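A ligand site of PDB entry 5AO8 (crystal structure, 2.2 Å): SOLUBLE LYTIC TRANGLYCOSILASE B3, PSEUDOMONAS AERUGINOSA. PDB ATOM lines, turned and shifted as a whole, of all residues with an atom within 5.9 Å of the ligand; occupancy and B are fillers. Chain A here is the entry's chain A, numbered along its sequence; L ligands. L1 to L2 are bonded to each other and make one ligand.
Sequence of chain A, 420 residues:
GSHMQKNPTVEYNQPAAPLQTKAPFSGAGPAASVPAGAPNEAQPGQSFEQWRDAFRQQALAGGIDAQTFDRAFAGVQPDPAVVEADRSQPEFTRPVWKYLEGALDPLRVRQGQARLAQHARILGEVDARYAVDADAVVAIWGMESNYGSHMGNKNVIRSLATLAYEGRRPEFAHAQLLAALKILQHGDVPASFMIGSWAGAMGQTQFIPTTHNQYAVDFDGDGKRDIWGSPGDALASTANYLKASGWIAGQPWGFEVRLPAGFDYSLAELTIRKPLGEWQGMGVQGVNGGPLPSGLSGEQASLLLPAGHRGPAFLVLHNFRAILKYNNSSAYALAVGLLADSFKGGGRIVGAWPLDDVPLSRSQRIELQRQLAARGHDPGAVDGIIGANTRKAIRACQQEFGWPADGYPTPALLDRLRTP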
ATOM      1  N   LYS A  98      28.635   3.811 -19.091  1.00  0.00           N
ATOM      2  CA  LYS A  98      29.829   3.767 -19.937  1.00  0.00           C
ATOM      3  C   LYS A  98      29.577   2.760 -21.050  1.00  0.00           C
ATOM      4  O   LYS A  98      29.768   3.033 -22.237  1.00  0.00           O
ATOM      5  CB  LYS A  98      31.094   3.404 -19.137  1.00  0.00           C
ATOM      6  CG  LYS A  98      32.402   3.328 -19.989  1.00  0.00           C
ATOM      7  CD  LYS A  98      32.766   4.671 -20.625  1.00  0.00           C
ATOM      8  CE  LYS A  98      33.822   4.533 -21.715  1.00  0.00           C
ATOM      9  NZ  LYS A  98      33.215   4.171 -23.028  1.00  0.00           N
ATOM     10  N   TYR A  99      29.168   1.575 -20.630  1.00  0.00           N
ATOM     11  CA  TYR A  99      28.763   0.503 -21.520  1.00  0.00           C
ATOM     12  C   TYR A  99      27.804   0.933 -22.620  1.00  0.00           C
ATOM     13  O   TYR A  99      27.888   0.416 -23.742  1.00  0.00           O
ATOM     14  CB  TYR A  99      28.105  -0.575 -20.696  1.00  0.00           C
ATOM     15  CG  TYR A  99      27.661  -1.739 -21.523  1.00  0.00           C
ATOM     16  CD1 TYR A  99      28.550  -2.723 -21.880  1.00  0.00           C
ATOM     17  CD2 TYR A  99      26.345  -1.865 -21.901  1.00  0.00           C
ATOM     18  CE1 TYR A  99      28.151  -3.799 -22.605  1.00  0.00           C
ATOM     19  CE2 TYR A  99      25.933  -2.936 -22.630  1.00  0.00           C
ATOM     20  CZ  TYR A  99      26.849  -3.908 -22.979  1.00  0.00           C
ATOM     21  OH  TYR A  99      26.468  -4.984 -23.717  1.00  0.00           O
ATOM     22  N   GLY A 102      29.557   3.029 -25.363  1.00  0.00           N
ATOM     23  CA  GLY A 102      30.237   2.166 -26.302  1.00  0.00           C
ATOM     24  C   GLY A 102      29.250   1.631 -27.290  1.00  0.00           C
ATOM     25  O   GLY A 102      29.405   1.773 -28.491  1.00  0.00           O
ATOM     26  N   ALA A 103      28.204   1.024 -26.772  1.00  0.00           N
ATOM     27  CA  ALA A 103      27.169   0.423 -27.579  1.00  0.00           C
ATOM     28  C   ALA A 103      26.557   1.361 -28.573  1.00  0.00           C
ATOM     29  O   ALA A 103      26.246   0.977 -29.686  1.00  0.00           O
ATOM     30  CB  ALA A 103      26.092  -0.118 -26.685  1.00  0.00           C
ATOM     31  N   ARG A 108      28.827   3.363 -34.581  1.00  0.00           N
ATOM     32  CA  ARG A 108      28.131   2.094 -34.714  1.00  0.00           C
ATOM     33  C   ARG A 108      26.696   2.296 -35.193  1.00  0.00           C
ATOM     34  O   ARG A 108      26.198   1.491 -35.980  1.00  0.00           O
ATOM     35  CB  ARG A 108      28.135   1.315 -33.401  1.00  0.00           C
ATOM     36  CG  ARG A 108      27.421   0.003 -33.504  1.00  0.00           C
ATOM     37  CD  ARG A 108      27.579  -0.716 -32.201  1.00  0.00           C
ATOM     38  NE  ARG A 108      28.859  -1.385 -32.130  1.00  0.00           N
ATOM     39  CZ  ARG A 108      29.554  -1.542 -31.018  1.00  0.00           C
ATOM     40  NH1 ARG A 108      29.107  -1.052 -29.878  1.00  0.00           N
ATOM     41  NH2 ARG A 108      30.703  -2.192 -31.051  1.00  0.00           N
ATOM     42  N   TRP A 141      23.429  -7.748 -34.262  1.00  0.00           N
ATOM     43  CA  TRP A 141      24.585  -7.888 -35.117  1.00  0.00           C
ATOM     44  C   TRP A 141      25.687  -6.862 -34.845  1.00  0.00           C
ATOM     45  O   TRP A 141      26.891  -7.184 -34.792  1.00  0.00           O
ATOM     46  CB  TRP A 141      24.109  -7.801 -36.572  1.00  0.00           C
ATOM     47  CG  TRP A 141      25.051  -8.260 -37.624  1.00  0.00           C
ATOM     48  CD1 TRP A 141      26.094  -9.168 -37.509  1.00  0.00           C
ATOM     49  CD2 TRP A 141      25.019  -7.861 -38.998  1.00  0.00           C
ATOM     50  NE1 TRP A 141      26.711  -9.330 -38.747  1.00  0.00           N
ATOM     51  CE2 TRP A 141      26.071  -8.545 -39.668  1.00  0.00           C
ATOM     52  CE3 TRP A 141      24.198  -6.987 -39.730  1.00  0.00           C
ATOM     53  CZ2 TRP A 141      26.313  -8.385 -41.032  1.00  0.00           C
ATOM     54  CZ3 TRP A 141      24.452  -6.817 -41.065  1.00  0.00           C
ATOM     55  CH2 TRP A 141      25.508  -7.521 -41.715  1.00  0.00           C
ATOM     56  N   GLY A 142      25.282  -5.611 -34.654  1.00  0.00           N
ATOM     57  CA  GLY A 142      26.223  -4.580 -34.227  1.00  0.00           C
ATOM     58  C   GLY A 142      26.819  -4.810 -32.867  1.00  0.00           C
ATOM     59  O   GLY A 142      28.030  -4.650 -32.680  1.00  0.00           O
ATOM     60  N   MET A 143      25.970  -5.166 -31.909  1.00  0.00           N
ATOM     61  CA  MET A 143      26.402  -5.463 -30.545  1.00  0.00           C
ATOM     62  C   MET A 143      27.349  -6.676 -30.438  1.00  0.00           C
ATOM     63  O   MET A 143      28.328  -6.698 -29.676  1.00  0.00           O
ATOM     64  CB  MET A 143      25.183  -5.714 -29.656  1.00  0.00           C
ATOM     65  CG  MET A 143      24.348  -4.460 -29.339  1.00  0.00           C
ATOM     66  SD  MET A 143      25.316  -3.168 -28.601  1.00  0.00           S
ATOM     67  CE  MET A 143      25.752  -3.951 -27.067  1.00  0.00           C
ATOM     68  N   GLU A 144      27.028  -7.717 -31.198  1.00  0.00           N
ATOM     69  CA  GLU A 144      27.759  -8.998 -31.102  1.00  0.00           C
ATOM     70  C   GLU A 144      29.120  -8.991 -31.799  1.00  0.00           C
ATOM     71  O   GLU A 144      30.101  -9.449 -31.256  1.00  0.00           O
ATOM     72  CB  GLU A 144      26.895 -10.116 -31.673  1.00  0.00           C
ATOM     73  CG  GLU A 144      25.712 -10.453 -30.794  1.00  0.00           C
ATOM     74  CD  GLU A 144      26.075 -10.880 -29.339  1.00  0.00           C
ATOM     75  OE1 GLU A 144      27.197 -11.394 -29.087  1.00  0.00           O
ATOM     76  OE2 GLU A 144      25.226 -10.696 -28.440  1.00  0.00           O
ATOM     77  N   SER A 145      29.180  -8.444 -33.000  1.00  0.00           N
ATOM     78  CA  SER A 145      30.401  -8.531 -33.772  1.00  0.00           C
ATOM     79  C   SER A 145      30.709  -7.242 -34.534  1.00  0.00           C
ATOM     80  O   SER A 145      31.489  -7.285 -35.457  1.00  0.00           O
ATOM     81  CB  SER A 145      30.286  -9.704 -34.766  1.00  0.00           C
ATOM     82  OG  SER A 145      29.297  -9.487 -35.763  1.00  0.00           O
ATOM     83  N   ASN A 146      30.091  -6.122 -34.147  1.00  0.00           N
ATOM     84  CA  ASN A 146      30.132  -4.896 -34.958  1.00  0.00           C
ATOM     85  C   ASN A 146      29.842  -5.142 -36.465  1.00  0.00           C
ATOM     86  O   ASN A 146      30.577  -4.696 -37.350  1.00  0.00           O
ATOM     87  CB  ASN A 146      31.472  -4.180 -34.780  1.00  0.00           C
ATOM     88  CG  ASN A 146      31.418  -2.749 -35.230  1.00  0.00           C
ATOM     89  OD1 ASN A 146      31.068  -1.871 -34.457  1.00  0.00           O
ATOM     90  ND2 ASN A 146      31.735  -2.506 -36.502  1.00  0.00           N
ATOM     91  N   HIS A 150      34.250  -7.397 -35.966  1.00  0.00           N
ATOM     92  CA  HIS A 150      34.982  -7.896 -34.798  1.00  0.00           C
ATOM     93  C   HIS A 150      34.315  -9.213 -34.356  1.00  0.00           C
ATOM     94  O   HIS A 150      33.569  -9.244 -33.379  1.00  0.00           O
ATOM     95  CB  HIS A 150      35.006  -6.901 -33.608  1.00  0.00           C
ATOM     96  CG  HIS A 150      35.805  -5.649 -33.832  1.00  0.00           C
ATOM     97  ND1 HIS A 150      35.493  -4.737 -34.808  1.00  0.00           N
ATOM     98  CD2 HIS A 150      36.874  -5.150 -33.177  1.00  0.00           C
ATOM     99  CE1 HIS A 150      36.343  -3.725 -34.757  1.00  0.00           C
ATOM    100  N   MET A 151      34.582 -10.279 -35.083  1.00  0.00           N
ATOM    101  CA  MET A 151      34.073 -11.594 -34.768  1.00  0.00           C
ATOM    102  C   MET A 151      34.885 -12.316 -33.738  1.00  0.00           C
ATOM    103  O   MET A 151      34.493 -13.346 -33.178  1.00  0.00           O
ATOM    104  CB  MET A 151      34.060 -12.456 -35.998  1.00  0.00           C
ATOM    105  CG  MET A 151      32.871 -12.295 -36.787  1.00  0.00           C
ATOM    106  SD  MET A 151      32.969 -13.337 -38.206  1.00  0.00           S
ATOM    107  CE  MET A 151      33.899 -12.276 -39.269  1.00  0.00           C
ATOM    108  N   GLY A 152      36.085 -11.820 -33.529  1.00  0.00           N
ATOM    109  CA  GLY A 152      36.964 -12.431 -32.577  1.00  0.00           C
ATOM    110  C   GLY A 152      38.042 -13.107 -33.371  1.00  0.00           C
ATOM    111  O   GLY A 152      37.948 -13.243 -34.585  1.00  0.00           O
ATOM    112  N   GLY A 196      35.880 -17.179 -33.345  1.00  0.00           N
ATOM    113  CA  GLY A 196      34.964 -16.599 -32.417  1.00  0.00           C
ATOM    114  C   GLY A 196      35.743 -16.041 -31.242  1.00  0.00           C
ATOM    115  O   GLY A 196      36.899 -15.717 -31.385  1.00  0.00           O
ATOM    116  N   SER A 197      35.078 -15.922 -30.110  1.00  0.00           N
ATOM    117  CA  SER A 197      35.607 -15.248 -28.939  1.00  0.00           C
ATOM    118  C   SER A 197      36.270 -16.259 -28.023  1.00  0.00           C
ATOM    119  O   SER A 197      36.070 -17.446 -28.208  1.00  0.00           O
ATOM    120  CB  SER A 197      34.467 -14.565 -28.199  1.00  0.00           C
ATOM    121  OG  SER A 197      33.680 -15.576 -27.572  1.00  0.00           O
ATOM    122  N   ALA A 201      31.934 -18.361 -28.405  1.00  0.00           N
ATOM    123  CA  ALA A 201      30.837 -17.693 -29.135  1.00  0.00           C
ATOM    124  C   ALA A 201      31.327 -17.371 -30.559  1.00  0.00           C
ATOM    125  O   ALA A 201      32.371 -16.752 -30.727  1.00  0.00           O
ATOM    126  CB  ALA A 201      30.400 -16.435 -28.406  1.00  0.00           C
ATOM    127  N   GLN A 206      27.793 -14.540 -32.835  1.00  0.00           N
ATOM    128  CA  GLN A 206      28.296 -14.984 -31.534  1.00  0.00           C
ATOM    129  C   GLN A 206      27.372 -16.036 -30.930  1.00  0.00           C
ATOM    130  O   GLN A 206      27.116 -16.038 -29.719  1.00  0.00           O
ATOM    131  CB  GLN A 206      28.513 -13.794 -30.605  1.00  0.00           C
ATOM    132  CG  GLN A 206      29.546 -12.813 -31.132  1.00  0.00           C
ATOM    133  CD  GLN A 206      31.004 -13.381 -31.094  1.00  0.00           C
ATOM    134  OE1 GLN A 206      31.613 -13.507 -30.030  1.00  0.00           O
ATOM    135  NE2 GLN A 206      31.532 -13.711 -32.256  1.00  0.00           N
ATOM    136  N   ASN A 327      21.239 -12.887 -24.739  1.00  0.00           N
ATOM    137  CA  ASN A 327      22.362 -12.523 -23.896  1.00  0.00           C
ATOM    138  C   ASN A 327      21.793 -11.972 -22.560  1.00  0.00           C
ATOM    139  O   ASN A 327      21.119 -10.906 -22.527  1.00  0.00           O
ATOM    140  CB  ASN A 327      23.220 -11.489 -24.578  1.00  0.00           C
ATOM    141  CG  ASN A 327      24.639 -11.503 -24.091  1.00  0.00           C
ATOM    142  OD1 ASN A 327      24.915 -11.132 -22.957  1.00  0.00           O
ATOM    143  ND2 ASN A 327      25.562 -11.917 -24.958  1.00  0.00           N
ATOM    144  N   TYR A 332      22.928  -5.157 -21.662  1.00  0.00           N
ATOM    145  CA  TYR A 332      22.967  -5.550 -23.065  1.00  0.00           C
ATOM    146  C   TYR A 332      21.628  -5.402 -23.709  1.00  0.00           C
ATOM    147  O   TYR A 332      21.565  -4.886 -24.785  1.00  0.00           O
ATOM    148  CB  TYR A 332      23.472  -6.984 -23.210  1.00  0.00           C
ATOM    149  CG  TYR A 332      23.367  -7.606 -24.580  1.00  0.00           C
ATOM    150  CD1 TYR A 332      22.201  -8.246 -24.983  1.00  0.00           C
ATOM    151  CD2 TYR A 332      24.428  -7.569 -25.450  1.00  0.00           C
ATOM    152  CE1 TYR A 332      22.100  -8.839 -26.257  1.00  0.00           C
ATOM    153  CE2 TYR A 332      24.344  -8.160 -26.722  1.00  0.00           C
ATOM    154  CZ  TYR A 332      23.178  -8.805 -27.101  1.00  0.00           C
ATOM    155  OH  TYR A 332      23.071  -9.411 -28.336  1.00  0.00           O
HETATM  156  C1  LIG L   1      32.960  -5.932 -25.008  1.00  0.00           C
HETATM  157  C2  LIG L   1      33.234  -3.631 -29.305  1.00  0.00           C
HETATM  158  N1  LIG L   1      35.547  -5.550 -24.843  1.00  0.00           N
HETATM  159  O1  LIG L   1      32.230  -7.477 -28.079  1.00  0.00           O
HETATM  160  O2  LIG L   1      32.027  -1.151 -26.998  1.00  0.00           O
HETATM  161  C3  LIG L   1      33.975  -2.142 -31.048  1.00  0.00           C
HETATM  162  C4  LIG L   1      32.085  -6.220 -23.821  1.00  0.00           C
HETATM  163  C5  LIG L   1      32.653  -3.767 -27.897  1.00  0.00           C
HETATM  164  C6  LIG L   1      34.170  -5.037 -24.628  1.00  0.00           C
HETATM  165  C7  LIG L   1      32.712  -5.222 -27.381  1.00  0.00           C
HETATM  166  C8  LIG L   1      32.029  -6.098 -28.402  1.00  0.00           C
HETATM  167  C9  LIG L   1      32.651  -5.805 -29.772  1.00  0.00           C
HETATM  168  C10 LIG L   1      31.942  -6.574 -30.824  1.00  0.00           C
HETATM  169  C11 LIG L   1      33.107  -1.623 -26.629  1.00  0.00           C
HETATM  170  C12 LIG L   1      34.136  -0.833 -25.724  1.00  0.00           C
HETATM  171  N2  LIG L   1      33.501  -2.968 -27.040  1.00  0.00           N
HETATM  172  O3  LIG L   1      34.024  -3.912 -24.165  1.00  0.00           O
HETATM  173  O4  LIG L   1      33.206  -2.287 -29.854  1.00  0.00           O
HETATM  174  O5  LIG L   1      32.117  -5.368 -26.061  1.00  0.00           O
HETATM  175  O6  LIG L   1      30.642  -5.939 -30.778  1.00  0.00           O
HETATM  176  O7  LIG L   1      32.489  -4.461 -30.125  1.00  0.00           O
HETATM  177  C1  LG2 L   2      31.004  -8.248 -27.977  1.00  0.00           C
HETATM  178  C2  LG2 L   2      31.414  -9.721 -28.029  1.00  0.00           C
HETATM  179  C3  LG2 L   2      30.231 -10.666 -27.795  1.00  0.00           C
HETATM  180  C4  LG2 L   2      29.373 -10.209 -26.606  1.00  0.00           C
HETATM  181  C5  LG2 L   2      29.066  -8.725 -26.765  1.00  0.00           C
HETATM  182  C6  LG2 L   2      28.147  -8.087 -25.719  1.00  0.00           C
HETATM  183  C7  LG2 L   2      33.317 -10.592 -29.384  1.00  0.00           C
HETATM  184  C8  LG2 L   2      33.932 -10.892 -30.756  1.00  0.00           C
HETATM  185  N1  LG2 L   2      31.996  -9.986 -29.304  1.00  0.00           N
HETATM  186  O1  LG2 L   2      30.698 -11.986 -27.555  1.00  0.00           O
HETATM  187  O2  LG2 L   2      28.210 -11.052 -26.662  1.00  0.00           O
HETATM  188  O3  LG2 L   2      30.315  -8.006 -26.791  1.00  0.00           O
HETATM  189  O4  LG2 L   2      28.760  -6.907 -25.206  1.00  0.00           O
HETATM  190  O5  LG2 L   2      33.888 -10.855 -28.371  1.00  0.00           O
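OH of Tyr 332 lies within hydrogen-bond range of OE2 of Glu 144 (2.5 Å). The side-chain hydroxyl (OG) of Ser 197 is in hydrogen-bond range of the backbone NH (N) of Ala 201. The side-chain amide oxygen (OD1) of Asn 146 sits at hydrogen-bond distance from the guanidinium group (NE) of Arg 108 (3.2 Å). The backbone carbonyl oxygen of Met 151 sits at hydrogen-bond distance from the side-chain amide nitrogen of Gln 206 (3.1 Å). The guanidinium group (NH1) of Arg 108 sits at hydrogen-bond distance from the backbone carbonyl oxygen (O) of Gly 102 (3.2 Å). The backbone carbonyl oxygen (O) of Ser 145 sits at hydrogen-bond distance from the backbone NH (N) of His 150, at 2.8 Å. The side-chain hydroxyl (OG) of Ser 145 sits at hydrogen-bond distance from the backbone carbonyl oxygen (O) of Trp 141 (3.5 Å). O of Trp 141 sits at hydrogen-bond distance from N of Asn 146 (3.4 Å).
Merely in contact with the ligand: His 150, Met 151, Gly 152, Ser 145, Ser 197, Tyr 332 and Gly 102. Hydrophobic or aromatic side chains within 4 Å of the ligand: Tyr 332. Of the 20 residues printed, 15 come within 4 Å of the ligand.
The side-chain hydroxyl (OH) of Tyr 99 sits at hydrogen-bond distance from an oxygen (O4) of LG2 L2, 3.3 Å away. The side-chain amide oxygen (OE1) of Gln 206 is in hydrogen-bond range of an oxygen (O1) of LG2 L2 (3.0 Å). An oxygen (O2) of LG2 L2 lies within hydrogen-bond range of the side-chain amide nitrogen (ND2) of Asn 327. The backbone carbonyl oxygen (O) of Met 143 sits at hydrogen-bond distance from an oxygen (O6) of LIG L1 (2.7 Å). NH2 of Arg 108 is in hydrogen-bond range of O4 of LIG L1 (2.8 Å). O of Glu 144 lies within hydrogen-bond range of N1 of LG2 L2 (2.8 Å). The backbone carbonyl oxygen (O) of Gly 142 sits at hydrogen-bond distance from an oxygen (O6) of LIG L1. An oxygen (O2) of LG2 L2 lies within hydrogen-bond range of the side-chain carboxylate (OE1) of Glu 144. An oxygen (O6) of LIG L1 lies within hydrogen-bond range of the backbone NH (N) of Asn 146.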
